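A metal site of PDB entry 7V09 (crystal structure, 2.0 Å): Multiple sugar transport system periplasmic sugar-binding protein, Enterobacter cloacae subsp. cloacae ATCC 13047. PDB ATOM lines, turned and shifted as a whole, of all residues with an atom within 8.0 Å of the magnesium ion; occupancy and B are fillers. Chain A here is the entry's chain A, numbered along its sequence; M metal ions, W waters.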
ATOM      1  N   VAL A 129      11.376 -13.765  -9.803  1.00  0.00           N
ATOM      2  CA  VAL A 129       9.967 -13.634  -9.473  1.00  0.00           C
ATOM      3  C   VAL A 129       9.192 -13.410 -10.772  1.00  0.00           C
ATOM      4  O   VAL A 129       9.277 -12.337 -11.376  1.00  0.00           O
ATOM      5  CB  VAL A 129       9.727 -12.503  -8.473  1.00  0.00           C
ATOM      6  CG1 VAL A 129       8.308 -12.578  -7.934  1.00  0.00           C
ATOM      7  CG2 VAL A 129      10.737 -12.556  -7.346  1.00  0.00           C
ATOM      8  N   TYR A 131       5.423 -13.291 -12.839  1.00  0.00           N
ATOM      9  CA  TYR A 131       4.092 -12.806 -12.512  1.00  0.00           C
ATOM     10  C   TYR A 131       3.226 -12.798 -13.767  1.00  0.00           C
ATOM     11  O   TYR A 131       3.737 -12.692 -14.889  1.00  0.00           O
ATOM     12  CB  TYR A 131       4.135 -11.399 -11.891  1.00  0.00           C
ATOM     13  CG  TYR A 131       4.533 -10.304 -12.858  1.00  0.00           C
ATOM     14  CD1 TYR A 131       5.875  -9.991 -13.067  1.00  0.00           C
ATOM     15  CD2 TYR A 131       3.571  -9.561 -13.543  1.00  0.00           C
ATOM     16  CE1 TYR A 131       6.241  -8.979 -13.939  1.00  0.00           C
ATOM     17  CE2 TYR A 131       3.941  -8.562 -14.417  1.00  0.00           C
ATOM     18  CZ  TYR A 131       5.271  -8.262 -14.611  1.00  0.00           C
ATOM     19  OH  TYR A 131       5.639  -7.272 -15.482  1.00  0.00           O
ATOM     20  N   LYS A 133       0.980 -10.818 -16.122  1.00  0.00           N
ATOM     21  CA  LYS A 133       0.895  -9.394 -16.428  1.00  0.00           C
ATOM     22  C   LYS A 133      -0.525  -8.869 -16.265  1.00  0.00           C
ATOM     23  O   LYS A 133      -0.727  -7.761 -15.748  1.00  0.00           O
ATOM     24  CB  LYS A 133       1.397  -9.131 -17.853  1.00  0.00           C
ATOM     25  CG  LYS A 133       2.853  -9.502 -18.080  1.00  0.00           C
ATOM     26  CD  LYS A 133       3.489  -8.586 -19.111  1.00  0.00           C
ATOM     27  CE  LYS A 133       4.219  -9.370 -20.188  1.00  0.00           C
ATOM     28  NZ  LYS A 133       5.697  -9.278 -20.033  1.00  0.00           N
ATOM     29  N   GLU A 143       5.265  -3.010 -11.964  1.00  0.00           N
ATOM     30  CA  GLU A 143       6.348  -3.949 -11.711  1.00  0.00           C
ATOM     31  C   GLU A 143       7.186  -3.465 -10.525  1.00  0.00           C
ATOM     32  O   GLU A 143       7.695  -2.340 -10.568  1.00  0.00           O
ATOM     33  CB  GLU A 143       7.220  -4.106 -12.950  1.00  0.00           C
ATOM     34  CG  GLU A 143       8.525  -4.860 -12.703  1.00  0.00           C
ATOM     35  CD  GLU A 143       9.024  -5.582 -13.937  1.00  0.00           C
ATOM     36  OE1 GLU A 143       8.180  -6.015 -14.757  1.00  0.00           O
ATOM     37  OE2 GLU A 143      10.253  -5.715 -14.091  1.00  0.00           O
ATOM     38  N   PRO A 144       7.319  -4.257  -9.463  1.00  0.00           N
ATOM     39  CA  PRO A 144       8.072  -3.787  -8.284  1.00  0.00           C
ATOM     40  C   PRO A 144       9.512  -3.447  -8.640  1.00  0.00           C
ATOM     41  O   PRO A 144      10.151  -4.117  -9.462  1.00  0.00           O
ATOM     42  CB  PRO A 144       8.003  -4.966  -7.316  1.00  0.00           C
ATOM     43  CG  PRO A 144       7.025  -5.934  -7.875  1.00  0.00           C
ATOM     44  CD  PRO A 144       6.599  -5.519  -9.234  1.00  0.00           C
ATOM     45  N   LEU A 261       3.518 -13.545 -19.425  1.00  0.00           N
ATOM     46  CA  LEU A 261       4.567 -13.808 -18.451  1.00  0.00           C
ATOM     47  C   LEU A 261       5.450 -12.574 -18.280  1.00  0.00           C
ATOM     48  O   LEU A 261       5.994 -12.059 -19.270  1.00  0.00           O
ATOM     49  CB  LEU A 261       5.403 -15.008 -18.871  1.00  0.00           C
ATOM     50  CG  LEU A 261       6.283 -15.604 -17.761  1.00  0.00           C
ATOM     51  CD1 LEU A 261       5.456 -15.935 -16.535  1.00  0.00           C
ATOM     52  CD2 LEU A 261       7.030 -16.837 -18.258  1.00  0.00           C
ATOM     53  N   GLY A 262       5.589 -12.113 -17.038  1.00  0.00           N
ATOM     54  CA  GLY A 262       6.486 -11.026 -16.711  1.00  0.00           C
ATOM     55  C   GLY A 262       7.583 -11.487 -15.762  1.00  0.00           C
ATOM     56  O   GLY A 262       7.526 -12.590 -15.202  1.00  0.00           O
ATOM     57  N   PHE A 263       8.579 -10.630 -15.592  1.00  0.00           N
ATOM     58  CA  PHE A 263       9.744 -10.962 -14.786  1.00  0.00           C
ATOM     59  C   PHE A 263      10.195  -9.738 -14.011  1.00  0.00           C
ATOM     60  O   PHE A 263      10.357  -8.650 -14.584  1.00  0.00           O
ATOM     61  CB  PHE A 263      10.889 -11.483 -15.660  1.00  0.00           C
ATOM     62  CG  PHE A 263      12.049 -12.041 -14.877  1.00  0.00           C
ATOM     63  CD1 PHE A 263      11.960 -13.282 -14.291  1.00  0.00           C
ATOM     64  CD2 PHE A 263      13.227 -11.323 -14.743  1.00  0.00           C
ATOM     65  CE1 PHE A 263      13.021 -13.806 -13.567  1.00  0.00           C
ATOM     66  CE2 PHE A 263      14.292 -11.829 -14.027  1.00  0.00           C
ATOM     67  CZ  PHE A 263      14.188 -13.075 -13.437  1.00  0.00           C
ATOM     68  N   VAL A 264      10.391  -9.902 -12.700  1.00  0.00           N
ATOM     69  CA  VAL A 264      10.974  -8.860 -11.866  1.00  0.00           C
ATOM     70  C   VAL A 264      12.192  -9.450 -11.161  1.00  0.00           C
ATOM     71  O   VAL A 264      12.257 -10.659 -10.894  1.00  0.00           O
ATOM     72  CB  VAL A 264       9.966  -8.283 -10.838  1.00  0.00           C
ATOM     73  CG1 VAL A 264       8.560  -8.274 -11.411  1.00  0.00           C
ATOM     74  CG2 VAL A 264      10.007  -9.051  -9.520  1.00  0.00           C
ATOM     75  N   VAL A 265      13.164  -8.594 -10.887  1.00  0.00           N
ATOM     76  CA  VAL A 265      14.416  -8.989 -10.234  1.00  0.00           C
ATOM     77  C   VAL A 265      14.382  -8.456  -8.802  1.00  0.00           C
ATOM     78  O   VAL A 265      14.214  -7.245  -8.600  1.00  0.00           O
ATOM     79  CB  VAL A 265      15.633  -8.444 -10.991  1.00  0.00           C
ATOM     80  CG1 VAL A 265      16.922  -8.835 -10.258  1.00  0.00           C
ATOM     81  CG2 VAL A 265      15.648  -8.968 -12.416  1.00  0.00           C
ATOM     82  N   LEU A 343      10.895 -11.036 -23.624  1.00  0.00           N
ATOM     83  CA  LEU A 343      11.279 -11.635 -22.341  1.00  0.00           C
ATOM     84  C   LEU A 343      12.597 -12.408 -22.414  1.00  0.00           C
ATOM     85  O   LEU A 343      13.422 -12.246 -21.502  1.00  0.00           O
ATOM     86  CB  LEU A 343      10.145 -12.521 -21.814  1.00  0.00           C
ATOM     87  CG  LEU A 343      10.347 -13.104 -20.417  1.00  0.00           C
ATOM     88  CD1 LEU A 343       9.669 -12.244 -19.365  1.00  0.00           C
ATOM     89  CD2 LEU A 343       9.839 -14.534 -20.363  1.00  0.00           C
ATOM     90  N   GLU A 346      15.234  -9.777 -22.257  1.00  0.00           N
ATOM     91  CA  GLU A 346      15.247  -9.162 -20.937  1.00  0.00           C
ATOM     92  C   GLU A 346      15.904 -10.082 -19.922  1.00  0.00           C
ATOM     93  O   GLU A 346      16.619  -9.630 -19.019  1.00  0.00           O
ATOM     94  CB  GLU A 346      13.832  -8.789 -20.512  1.00  0.00           C
ATOM     95  CG  GLU A 346      13.631  -8.658 -19.016  1.00  0.00           C
ATOM     96  CD  GLU A 346      12.187  -8.389 -18.635  1.00  0.00           C
ATOM     97  OE1 GLU A 346      11.299  -8.567 -19.501  1.00  0.00           O
ATOM     98  OE2 GLU A 346      11.936  -7.989 -17.471  1.00  0.00           O
ATOM     99  N   LEU A 347      15.668 -11.390 -20.045  1.00  0.00           N
ATOM    100  CA  LEU A 347      16.344 -12.355 -19.184  1.00  0.00           C
ATOM    101  C   LEU A 347      17.843 -12.399 -19.492  1.00  0.00           C
ATOM    102  O   LEU A 347      18.660 -12.449 -18.571  1.00  0.00           O
ATOM    103  CB  LEU A 347      15.719 -13.743 -19.352  1.00  0.00           C
ATOM    104  CG  LEU A 347      14.289 -13.912 -18.848  1.00  0.00           C
ATOM    105  CD1 LEU A 347      13.697 -15.228 -19.325  1.00  0.00           C
ATOM    106  CD2 LEU A 347      14.251 -13.830 -17.332  1.00  0.00           C
ATOM    107  N   GLN A 350      19.782  -9.664 -17.982  1.00  0.00           N
ATOM    108  CA  GLN A 350      19.982  -9.758 -16.546  1.00  0.00           C
ATOM    109  C   GLN A 350      21.211 -10.589 -16.171  1.00  0.00           C
ATOM    110  O   GLN A 350      21.430 -10.840 -14.978  1.00  0.00           O
ATOM    111  CB  GLN A 350      18.738 -10.354 -15.887  1.00  0.00           C
ATOM    112  CG  GLN A 350      17.638  -9.341 -15.611  1.00  0.00           C
ATOM    113  CD  GLN A 350      18.172  -8.042 -15.035  1.00  0.00           C
ATOM    114  OE1 GLN A 350      18.846  -8.043 -14.004  1.00  0.00           O
ATOM    115  NE2 GLN A 350      17.879  -6.933 -15.699  1.00  0.00           N
HETATM  116 MG    MG M   1      10.363  -7.100 -16.038  1.00  0.00          MG
HETATM  117  O   HOH W   1      11.007  -5.140 -17.059  1.00  0.00           O
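The side-chain carboxylate (OE1) of Glu 143 sits at hydrogen-bond distance from the side-chain hydroxyl (OH) of Tyr 131 (2.9 Å).
Within 4 Å of the magnesium ion: Glu 143, Phe 263 and Glu 346.
The magnesium ion is bound by O of Phe 263 (2.1 Å), water W1 (2.3 Å), OE2 of Glu 346 (2.3 Å) and OE2 of Glu 143 (2.4 Å).
Slightly farther from the magnesium ion lies OE1 of Glu 143 (2.8 Å).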
